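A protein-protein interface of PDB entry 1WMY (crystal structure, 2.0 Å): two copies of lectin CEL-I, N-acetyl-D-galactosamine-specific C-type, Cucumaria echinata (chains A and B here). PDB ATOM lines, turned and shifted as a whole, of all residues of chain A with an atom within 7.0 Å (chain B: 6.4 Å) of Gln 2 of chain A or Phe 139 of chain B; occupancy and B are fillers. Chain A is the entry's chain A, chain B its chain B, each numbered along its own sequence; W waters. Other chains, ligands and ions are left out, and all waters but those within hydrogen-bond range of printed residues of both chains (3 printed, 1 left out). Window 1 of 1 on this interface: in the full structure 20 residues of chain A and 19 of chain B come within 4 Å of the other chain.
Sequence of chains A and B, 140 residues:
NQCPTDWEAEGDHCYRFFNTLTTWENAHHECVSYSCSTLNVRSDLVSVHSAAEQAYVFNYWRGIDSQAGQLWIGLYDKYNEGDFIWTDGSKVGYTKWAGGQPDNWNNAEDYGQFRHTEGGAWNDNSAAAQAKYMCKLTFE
Of the 10 printed residues of chain A, 9 touch a printed residue of chain B.
Hydrophobic or aromatic side chains of chain A that line the printed part of chain B: Pro 4, Ala 9 and Phe 139.
Printed residues of chain B that touch a printed residue of chain A: Asn 1, Gln 2, Cys 3, Pro 4, Ala 9, Gly 11, Asp 12, His 13, Cys 14, Leu 39, Phe 139 and Glu 140.
Hydrophobic or aromatic side chains of chain B within 4 Å of the printed part of chain A: Pro 4, Ala 9, Leu 39 and Phe 139.
Among the printed residues, 22 pairs touch across the chains.
Of chain B, only Asn 1 (3.4 Å), Gln 2 (3.0 Å), Cys 3 (3.7 Å), Ala 9 (3.9 Å), Gly 11 (2.8 Å), His 13 (3.7 Å), Cys 14 (3.9 Å) and Phe 139 (3.1 Å) come within 4 Å of Gln 2 of chain A.
Of the printed residues of chain B, Pro 4 of chain A touches Leu 39 (3.3 Å) and Phe 139 (3.9 Å).
Of the printed residues of chain B, Ala 9 of chain A touches Gln 2 (3.8 Å).
Of the printed residues of chain A, Cys 3 of chain B touches Gln 2 and Phe 139.
Printed residues of chain A within 4 Å of Pro 4 of chain B: Leu 39 (3.5 Å) and Phe 139 (3.9 Å).
Of chain A, only Gln 2, Cys 3, Pro 4 and Thr 5 come within 4 Å of Phe 139 of chain B.
The nearest residue of chain B that does not touch Gln 2 of chain A is Glu 10 of chain B (4.4 Å).
The nearest printed residue of chain B that does not touch Phe 139 of chain A is Asn 1 of chain B (5.3 Å).
OD1 of Asn 1 of chain B is in hydrogen-bond range of N of Cys 3 of chain B, at 3.0 Å.
O of Leu 137 of chain B sits at hydrogen-bond distance from ND1 of His 13 of chain B, at 2.8 Å.
The side-chain sulfur of Cys 3 of chain A is disulfide-bonded to the side-chain sulfur of Cys 14 of chain A, 2.0 Å away.
The side-chain sulfur (SG) of Cys 3 of chain B lies close to the backbone NH (N) of Ala 9 of chain B (3.7 Å).
The backbone NH of Leu 137 of chain B lies within hydrogen-bond range of the backbone carbonyl oxygen of Cys 14 of chain B.
The backbone carbonyl oxygen (O) of Cys 14 of chain A sits at hydrogen-bond distance from the backbone NH (N) of Leu 137 of chain A (2.8 Å).
NE2 of Gln 2 of chain A lies within hydrogen-bond range of O of Gly 11 of chain B (2.8 Å).
The side-chain hydroxyl (OG1) of Thr 5 of chain A sits at hydrogen-bond distance from the chain-end carboxylate (O) of Glu 140 of chain B (2.8 Å).
OE1 of Gln 2 of chain B sits at hydrogen-bond distance from N of Gln 2 of chain A (3.0 Å).
Water W2 lies within hydrogen-bond range of O of Thr 5 of chain A, ND2 of Asn 40 of chain B and O of Leu 39 of chain B.
Water W3 lies within hydrogen-bond range of O of Gln 2 of chain B (2.7 Å) and O of Gln 2 of chain A (2.8 Å).
Water W1 lies within hydrogen-bond range of OE1 of Gln 2 of chain A (2.8 Å), N of Asn 1 of chain B (3.1 Å), OE1 of Gln 2 of chain B (3.2 Å) and N of Asn 1 of chain A (3.2 Å).
Gln 2 of chain A touches its own counterpart, Gln 2 of chain B.
Gln 2 of chain A touches Cys 3 of chain B, and with the chains exchanged Cys 3 of chain A touches Gln 2 of chain B.
Gln 2 of chain A touches Cys 14 of chain B, and with the chains exchanged Cys 14 of chain A touches Gln 2 of chain B.
Pro 4 of chain A touches Leu 39 of chain B, and with the chains exchanged Leu 39 of chain A touches Pro 4 of chain B.
9 positions are printed for both chains.
Of the 22 pairs that touch across the chains among the printed residues, 17 have their exchanged pair printed and touching as well.
Among the printed residues, pairs that only touch across the chains: Phe 139 of chain A with Gln 2 of chain B, Gln 2 of chain A with Phe 139 of chain B, Pro 4 of chain A with Leu 39 of chain B, Gln 2 of chain A with Asn 1 of chain B, Asn 1 of chain A with Gln 2 of chain B, Leu 39 of chain A with Pro 4 of chain B, Gln 2 of chain A with His 13 of chain B, Gln 2 of chain A with Cys 3 of chain B, Cys 3 of chain A with Gln 2 of chain B, Thr 5 of chain A with Phe 139 of chain B, Ala 9 of chain A with Gln 2 of chain B, Phe 139 of chain A with Cys 3 of chain B, Cys 3 of chain A with Phe 139 of chain B, Gln 2 of chain A with Cys 14 of chain B, Cys 14 of chain A with Gln 2 of chain B, Gln 2 of chain A with Ala 9 of chain B, Asn 1 of chain A with Asp 12 of chain B, Pro 4 of chain A with Phe 139 of chain B and Phe 139 of chain A with Pro 4 of chain B.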
ATOM      1  N   ASN A   1      -7.195  -2.566 -17.872  1.00  0.00           N
ATOM      2  CA  ASN A   1      -7.286  -1.139 -18.161  1.00  0.00           C
ATOM      3  C   ASN A   1      -8.472  -0.520 -17.405  1.00  0.00           C
ATOM      4  O   ASN A   1      -9.619  -0.776 -17.730  1.00  0.00           O
ATOM      5  CB  ASN A   1      -7.444  -1.016 -19.659  1.00  0.00           C
ATOM      6  CG  ASN A   1      -7.419   0.415 -20.155  1.00  0.00           C
ATOM      7  OD1 ASN A   1      -7.958   1.339 -19.514  1.00  0.00           O
ATOM      8  ND2 ASN A   1      -6.808   0.602 -21.304  1.00  0.00           N
ATOM      9  N   GLN A   2      -8.194   0.342 -16.421  1.00  0.00           N
ATOM     10  CA  GLN A   2      -9.258   1.073 -15.733  1.00  0.00           C
ATOM     11  C   GLN A   2      -9.206   2.589 -15.977  1.00  0.00           C
ATOM     12  O   GLN A   2      -9.620   3.388 -15.169  1.00  0.00           O
ATOM     13  CB  GLN A   2      -9.210   0.760 -14.221  1.00  0.00           C
ATOM     14  CG  GLN A   2      -9.407  -0.729 -13.927  1.00  0.00           C
ATOM     15  CD  GLN A   2      -8.142  -1.632 -14.118  1.00  0.00           C
ATOM     16  OE1 GLN A   2      -7.041  -1.176 -13.966  1.00  0.00           O
ATOM     17  NE2 GLN A   2      -8.342  -2.889 -14.530  1.00  0.00           N
ATOM     18  N   CYS A   3      -8.678   2.981 -17.116  1.00  0.00           N
ATOM     19  CA  CYS A   3      -8.616   4.382 -17.449  1.00  0.00           C
ATOM     20  C   CYS A   3     -10.001   4.909 -17.942  1.00  0.00           C
ATOM     21  O   CYS A   3     -10.732   4.198 -18.621  1.00  0.00           O
ATOM     22  CB  CYS A   3      -7.520   4.625 -18.504  1.00  0.00           C
ATOM     23  SG  CYS A   3      -5.876   4.695 -17.806  1.00  0.00           S
ATOM     24  N   PRO A   4     -10.343   6.156 -17.608  1.00  0.00           N
ATOM     25  CA  PRO A   4     -11.516   6.802 -18.224  1.00  0.00           C
ATOM     26  C   PRO A   4     -11.463   6.737 -19.771  1.00  0.00           C
ATOM     27  O   PRO A   4     -10.389   6.704 -20.365  1.00  0.00           O
ATOM     28  CB  PRO A   4     -11.429   8.267 -17.714  1.00  0.00           C
ATOM     29  CG  PRO A   4     -10.678   8.136 -16.415  1.00  0.00           C
ATOM     30  CD  PRO A   4      -9.716   7.035 -16.605  1.00  0.00           C
ATOM     31  N   THR A   5     -12.631   6.800 -20.395  1.00  0.00           N
ATOM     32  CA  THR A   5     -12.708   6.837 -21.824  1.00  0.00           C
ATOM     33  C   THR A   5     -11.907   8.026 -22.367  1.00  0.00           C
ATOM     34  O   THR A   5     -11.951   9.137 -21.804  1.00  0.00           O
ATOM     35  CB  THR A   5     -14.201   6.944 -22.241  1.00  0.00           C
ATOM     36  OG1 THR A   5     -14.885   5.747 -21.880  1.00  0.00           O
ATOM     37  CG2 THR A   5     -14.312   6.944 -23.739  1.00  0.00           C
ATOM     38  N   ALA A   9      -3.890   4.066 -21.022  1.00  0.00           N
ATOM     39  CA  ALA A   9      -3.414   3.398 -19.837  1.00  0.00           C
ATOM     40  C   ALA A   9      -1.938   3.065 -20.041  1.00  0.00           C
ATOM     41  O   ALA A   9      -1.564   2.519 -21.109  1.00  0.00           O
ATOM     42  CB  ALA A   9      -4.266   2.083 -19.614  1.00  0.00           C
ATOM     43  N   CYS A  14      -2.909   7.243 -16.280  1.00  0.00           N
ATOM     44  CA  CYS A  14      -3.661   7.406 -17.537  1.00  0.00           C
ATOM     45  C   CYS A  14      -3.118   8.660 -18.175  1.00  0.00           C
ATOM     46  O   CYS A  14      -2.761   9.573 -17.464  1.00  0.00           O
ATOM     47  CB  CYS A  14      -5.139   7.535 -17.244  1.00  0.00           C
ATOM     48  SG  CYS A  14      -5.863   6.144 -16.380  1.00  0.00           S
ATOM     49  N   LEU A  39     -12.774  10.918  -5.965  1.00  0.00           N
ATOM     50  CA  LEU A  39     -11.933   9.725  -6.067  1.00  0.00           C
ATOM     51  C   LEU A  39     -10.397   9.993  -5.911  1.00  0.00           C
ATOM     52  O   LEU A  39      -9.600   9.121  -6.183  1.00  0.00           O
ATOM     53  CB  LEU A  39     -12.177   9.085  -7.432  1.00  0.00           C
ATOM     54  CG  LEU A  39     -13.499   8.327  -7.603  1.00  0.00           C
ATOM     55  CD1 LEU A  39     -13.689   7.992  -9.070  1.00  0.00           C
ATOM     56  CD2 LEU A  39     -13.640   7.108  -6.736  1.00  0.00           C
ATOM     57  N   LEU A 137      -3.218  11.419 -15.363  1.00  0.00           N
ATOM     58  CA  LEU A 137      -3.924  11.175 -14.128  1.00  0.00           C
ATOM     59  C   LEU A 137      -3.004  10.507 -13.113  1.00  0.00           C
ATOM     60  O   LEU A 137      -2.297   9.593 -13.453  1.00  0.00           O
ATOM     61  CB  LEU A 137      -5.086  10.265 -14.369  1.00  0.00           C
ATOM     62  CG  LEU A 137      -6.180  10.793 -15.306  1.00  0.00           C
ATOM     63  CD1 LEU A 137      -7.263   9.687 -15.277  1.00  0.00           C
ATOM     64  CD2 LEU A 137      -6.653  12.171 -14.909  1.00  0.00           C
ATOM     65  N   PHE A 139      -3.404   8.794  -9.277  1.00  0.00           N
ATOM     66  CA  PHE A 139      -4.352   8.284  -8.266  1.00  0.00           C
ATOM     67  C   PHE A 139      -3.758   8.479  -6.882  1.00  0.00           C
ATOM     68  O   PHE A 139      -2.954   7.685  -6.401  1.00  0.00           O
ATOM     69  CB  PHE A 139      -4.701   6.858  -8.622  1.00  0.00           C
ATOM     70  CG  PHE A 139      -5.241   6.739 -10.008  1.00  0.00           C
ATOM     71  CD1 PHE A 139      -4.446   6.319 -11.034  1.00  0.00           C
ATOM     72  CD2 PHE A 139      -6.517   7.169 -10.308  1.00  0.00           C
ATOM     73  CE1 PHE A 139      -4.944   6.278 -12.321  1.00  0.00           C
ATOM     74  CE2 PHE A 139      -7.003   7.127 -11.578  1.00  0.00           C
ATOM     75  CZ  PHE A 139      -6.213   6.679 -12.590  1.00  0.00           C
ATOM     76  N   ASN B   1      -3.074  -1.387 -13.327  1.00  0.00           N
ATOM     77  CA  ASN B   1      -4.038  -0.983 -12.315  1.00  0.00           C
ATOM     78  C   ASN B   1      -4.102   0.502 -12.270  1.00  0.00           C
ATOM     79  O   ASN B   1      -3.281   1.188 -11.683  1.00  0.00           O
ATOM     80  CB  ASN B   1      -3.578  -1.474 -10.996  1.00  0.00           C
ATOM     81  CG  ASN B   1      -4.628  -1.289  -9.919  1.00  0.00           C
ATOM     82  OD1 ASN B   1      -5.388  -0.316  -9.892  1.00  0.00           O
ATOM     83  ND2 ASN B   1      -4.652  -2.225  -9.006  1.00  0.00           N
ATOM     84  N   GLN B   2      -5.120   1.013 -12.903  1.00  0.00           N
ATOM     85  CA  GLN B   2      -5.362   2.422 -12.876  1.00  0.00           C
ATOM     86  C   GLN B   2      -6.586   2.797 -11.978  1.00  0.00           C
ATOM     87  O   GLN B   2      -7.229   3.805 -12.190  1.00  0.00           O
ATOM     88  CB  GLN B   2      -5.542   2.890 -14.304  1.00  0.00           C
ATOM     89  CG  GLN B   2      -4.288   2.646 -15.148  1.00  0.00           C
ATOM     90  CD  GLN B   2      -4.229   1.268 -15.730  1.00  0.00           C
ATOM     91  OE1 GLN B   2      -5.223   0.733 -16.151  1.00  0.00           O
ATOM     92  NE2 GLN B   2      -3.044   0.686 -15.754  1.00  0.00           N
ATOM     93  N   CYS B   3      -6.912   1.963 -10.982  1.00  0.00           N
ATOM     94  CA  CYS B   3      -7.996   2.306 -10.028  1.00  0.00           C
ATOM     95  C   CYS B   3      -7.571   3.354  -8.999  1.00  0.00           C
ATOM     96  O   CYS B   3      -6.414   3.368  -8.559  1.00  0.00           O
ATOM     97  CB  CYS B   3      -8.500   1.057  -9.269  1.00  0.00           C
ATOM     98  SG  CYS B   3      -9.453  -0.060 -10.304  1.00  0.00           S
ATOM     99  N   PRO B   4      -8.515   4.176  -8.570  1.00  0.00           N
ATOM    100  CA  PRO B   4      -8.270   5.105  -7.448  1.00  0.00           C
ATOM    101  C   PRO B   4      -7.832   4.380  -6.217  1.00  0.00           C
ATOM    102  O   PRO B   4      -8.186   3.143  -6.044  1.00  0.00           O
ATOM    103  CB  PRO B   4      -9.610   5.815  -7.240  1.00  0.00           C
ATOM    104  CG  PRO B   4     -10.305   5.716  -8.588  1.00  0.00           C
ATOM    105  CD  PRO B   4      -9.870   4.299  -9.105  1.00  0.00           C
ATOM    106  N   ALA B   9      -9.011  -3.295  -8.475  1.00  0.00           N
ATOM    107  CA  ALA B   9      -9.147  -3.471  -9.920  1.00  0.00           C
ATOM    108  C   ALA B   9      -9.537  -4.902 -10.290  1.00  0.00           C
ATOM    109  O   ALA B   9      -8.981  -5.849  -9.758  1.00  0.00           O
ATOM    110  CB  ALA B   9      -7.806  -3.180 -10.578  1.00  0.00           C
ATOM    111  N   GLU B  10     -10.438  -5.032 -11.259  1.00  0.00           N
ATOM    112  CA  GLU B  10     -10.779  -6.332 -11.837  1.00  0.00           C
ATOM    113  C   GLU B  10     -11.508  -6.118 -13.147  1.00  0.00           C
ATOM    114  O   GLU B  10     -12.578  -5.487 -13.186  1.00  0.00           O
ATOM    115  CB  GLU B  10     -11.651  -7.095 -10.870  1.00  0.00           C
ATOM    116  CG  GLU B  10     -12.141  -8.411 -11.412  1.00  0.00           C
ATOM    117  CD  GLU B  10     -11.039  -9.448 -11.477  1.00  0.00           C
ATOM    118  OE1 GLU B  10      -9.869  -9.267 -10.959  1.00  0.00           O
ATOM    119  OE2 GLU B  10     -11.400 -10.482 -12.034  1.00  0.00           O
ATOM    120  N   GLY B  11     -10.913  -6.555 -14.246  1.00  0.00           N
ATOM    121  CA  GLY B  11     -11.515  -6.345 -15.547  1.00  0.00           C
ATOM    122  C   GLY B  11     -11.558  -4.864 -15.899  1.00  0.00           C
ATOM    123  O   GLY B  11     -10.614  -4.102 -15.637  1.00  0.00           O
ATOM    124  N   ASP B  12     -12.632  -4.423 -16.482  1.00  0.00           N
ATOM    125  CA  ASP B  12     -12.754  -3.022 -16.785  1.00  0.00           C
ATOM    126  C   ASP B  12     -13.370  -2.181 -15.654  1.00  0.00           C
ATOM    127  O   ASP B  12     -13.886  -1.112 -15.915  1.00  0.00           O
ATOM    128  CB  ASP B  12     -13.585  -2.785 -18.027  1.00  0.00           C
ATOM    129  CG  ASP B  12     -13.015  -3.403 -19.250  1.00  0.00           C
ATOM    130  OD1 ASP B  12     -11.762  -3.553 -19.395  1.00  0.00           O
ATOM    131  OD2 ASP B  12     -13.828  -3.812 -20.101  1.00  0.00           O
ATOM    132  N   HIS B  13     -13.314  -2.661 -14.431  1.00  0.00           N
ATOM    133  CA  HIS B  13     -13.963  -2.004 -13.314  1.00  0.00           C
ATOM    134  C   HIS B  13     -13.059  -1.886 -12.098  1.00  0.00           C
ATOM    135  O   HIS B  13     -11.983  -2.532 -12.022  1.00  0.00           O
ATOM    136  CB  HIS B  13     -15.214  -2.780 -12.967  1.00  0.00           C
ATOM    137  CG  HIS B  13     -16.245  -2.769 -14.055  1.00  0.00           C
ATOM    138  ND1 HIS B  13     -17.018  -1.667 -14.349  1.00  0.00           N
ATOM    139  CD2 HIS B  13     -16.594  -3.736 -14.945  1.00  0.00           C
ATOM    140  CE1 HIS B  13     -17.791  -1.954 -15.384  1.00  0.00           C
ATOM    141  NE2 HIS B  13     -17.566  -3.214 -15.747  1.00  0.00           N
ATOM    142  N   CYS B  14     -13.460  -0.988 -11.185  1.00  0.00           N
ATOM    143  CA  CYS B  14     -12.890  -0.891  -9.852  1.00  0.00           C
ATOM    144  C   CYS B  14     -14.031  -1.124  -8.869  1.00  0.00           C
ATOM    145  O   CYS B  14     -15.189  -0.743  -9.148  1.00  0.00           O
ATOM    146  CB  CYS B  14     -12.271   0.500  -9.607  1.00  0.00           C
ATOM    147  SG  CYS B  14     -11.058   1.057 -10.841  1.00  0.00           S
ATOM    148  N   LEU B  39     -14.412  12.884 -15.703  1.00  0.00           N
ATOM    149  CA  LEU B  39     -13.819  11.697 -16.252  1.00  0.00           C
ATOM    150  C   LEU B  39     -14.819  10.667 -16.693  1.00  0.00           C
ATOM    151  O   LEU B  39     -14.451   9.568 -17.095  1.00  0.00           O
ATOM    152  CB  LEU B  39     -12.877  11.081 -15.227  1.00  0.00           C
ATOM    153  CG  LEU B  39     -11.727  12.029 -14.833  1.00  0.00           C
ATOM    154  CD1 LEU B  39     -10.977  11.472 -13.584  1.00  0.00           C
ATOM    155  CD2 LEU B  39     -10.782  12.283 -16.011  1.00  0.00           C
ATOM    156  N   ASN B  40     -16.061  11.048 -16.769  1.00  0.00           N
ATOM    157  CA  ASN B  40     -17.139  10.177 -17.179  1.00  0.00           C
ATOM    158  C   ASN B  40     -17.167   8.884 -16.420  1.00  0.00           C
ATOM    159  O   ASN B  40     -17.461   7.815 -17.004  1.00  0.00           O
ATOM    160  CB  ASN B  40     -17.094   9.916 -18.678  1.00  0.00           C
ATOM    161  CG  ASN B  40     -17.351  11.157 -19.458  1.00  0.00           C
ATOM    162  OD1 ASN B  40     -18.432  11.728 -19.354  1.00  0.00           O
ATOM    163  ND2 ASN B  40     -16.351  11.619 -20.195  1.00  0.00           N
ATOM    164  N   VAL B  41     -16.828   8.950 -15.140  1.00  0.00           N
ATOM    165  CA  VAL B  41     -16.817   7.797 -14.274  1.00  0.00           C
ATOM    166  C   VAL B  41     -18.145   7.765 -13.475  1.00  0.00           C
ATOM    167  O   VAL B  41     -18.505   8.727 -12.780  1.00  0.00           O
ATOM    168  CB  VAL B  41     -15.655   7.871 -13.260  1.00  0.00           C
ATOM    169  CG1 VAL B  41     -15.729   6.662 -12.332  1.00  0.00           C
ATOM    170  CG2 VAL B  41     -14.262   7.896 -13.948  1.00  0.00           C
ATOM    171  N   ARG B  42     -18.854   6.667 -13.560  1.00  0.00           N
ATOM    172  CA  ARG B  42     -20.075   6.469 -12.830  1.00  0.00           C
ATOM    173  C   ARG B  42     -19.819   5.477 -11.725  1.00  0.00           C
ATOM    174  O   ARG B  42     -19.426   4.326 -11.987  1.00  0.00           O
ATOM    175  CB  ARG B  42     -21.231   5.961 -13.739  1.00  0.00           C
ATOM    176  CG  ARG B  42     -21.191   6.443 -15.177  1.00  0.00           C
ATOM    177  CD  ARG B  42     -21.341   7.960 -15.295  1.00  0.00           C
ATOM    178  NE  ARG B  42     -21.179   8.395 -16.660  1.00  0.00           N
ATOM    179  CZ  ARG B  42     -20.837   9.604 -17.035  1.00  0.00           C
ATOM    180  NH1 ARG B  42     -20.610  10.567 -16.180  1.00  0.00           N
ATOM    181  NH2 ARG B  42     -20.683   9.841 -18.328  1.00  0.00           N
ATOM    182  N   LEU B 137     -17.039   1.121  -9.994  1.00  0.00           N
ATOM    183  CA  LEU B 137     -16.816   2.158 -10.976  1.00  0.00           C
ATOM    184  C   LEU B 137     -16.997   1.654 -12.390  1.00  0.00           C
ATOM    185  O   LEU B 137     -16.479   0.603 -12.738  1.00  0.00           O
ATOM    186  CB  LEU B 137     -15.433   2.805 -10.826  1.00  0.00           C
ATOM    187  CG  LEU B 137     -15.053   3.387  -9.477  1.00  0.00           C
ATOM    188  CD1 LEU B 137     -13.618   3.950  -9.489  1.00  0.00           C
ATOM    189  CD2 LEU B 137     -16.102   4.447  -9.000  1.00  0.00           C
ATOM    190  N   THR B 138     -17.728   2.454 -13.221  1.00  0.00           N
ATOM    191  CA  THR B 138     -17.908   2.133 -14.616  1.00  0.00           C
ATOM    192  C   THR B 138     -17.400   3.315 -15.376  1.00  0.00           C
ATOM    193  O   THR B 138     -17.817   4.429 -15.109  1.00  0.00           O
ATOM    194  CB  THR B 138     -19.421   1.826 -14.927  1.00  0.00           C
ATOM    195  OG1 THR B 138     -19.838   0.628 -14.242  1.00  0.00           O
ATOM    196  CG2 THR B 138     -19.689   1.631 -16.436  1.00  0.00           C
ATOM    197  N   PHE B 139     -16.409   3.089 -16.249  1.00  0.00           N
ATOM    198  CA  PHE B 139     -15.789   4.147 -17.035  1.00  0.00           C
ATOM    199  C   PHE B 139     -16.582   4.251 -18.322  1.00  0.00           C
ATOM    200  O   PHE B 139     -16.332   3.529 -19.252  1.00  0.00           O
ATOM    201  CB  PHE B 139     -14.330   3.795 -17.281  1.00  0.00           C
ATOM    202  CG  PHE B 139     -13.577   3.646 -16.005  1.00  0.00           C
ATOM    203  CD1 PHE B 139     -13.425   2.405 -15.397  1.00  0.00           C
ATOM    204  CD2 PHE B 139     -13.166   4.737 -15.337  1.00  0.00           C
ATOM    205  CE1 PHE B 139     -12.812   2.285 -14.180  1.00  0.00           C
ATOM    206  CE2 PHE B 139     -12.452   4.600 -14.088  1.00  0.00           C
ATOM    207  CZ  PHE B 139     -12.308   3.390 -13.533  1.00  0.00           C
ATOM    208  N   GLU B 140     -17.571   5.143 -18.345  1.00  0.00           N
ATOM    209  CA  GLU B 140     -18.476   5.268 -19.530  1.00  0.00           C
ATOM    210  C   GLU B 140     -17.787   6.003 -20.672  1.00  0.00           C
ATOM    211  O   GLU B 140     -16.946   6.880 -20.420  1.00  0.00           O
ATOM    212  CB  GLU B 140     -19.779   5.979 -19.166  1.00  0.00           C
ATOM    213  CG  GLU B 140     -20.876   5.882 -20.253  1.00  0.00           C
ATOM    214  CD  GLU B 140     -22.209   6.516 -19.852  1.00  0.00           C
ATOM    215  OE1 GLU B 140     -23.132   6.538 -20.728  1.00  0.00           O
ATOM    216  OE2 GLU B 140     -22.335   7.027 -18.706  1.00  0.00           O
ATOM    217  OXT GLU B 140     -18.154   5.686 -21.804  1.00  0.00           O
HETATM  218  O   HOH W   1      -5.018  -2.368 -15.508  1.00  0.00           O
HETATM  219  O   HOH W   2     -13.591  10.409 -20.243  1.00  0.00           O
HETATM  220  O   HOH W   3      -9.415   5.139 -12.977  1.00  0.00           O
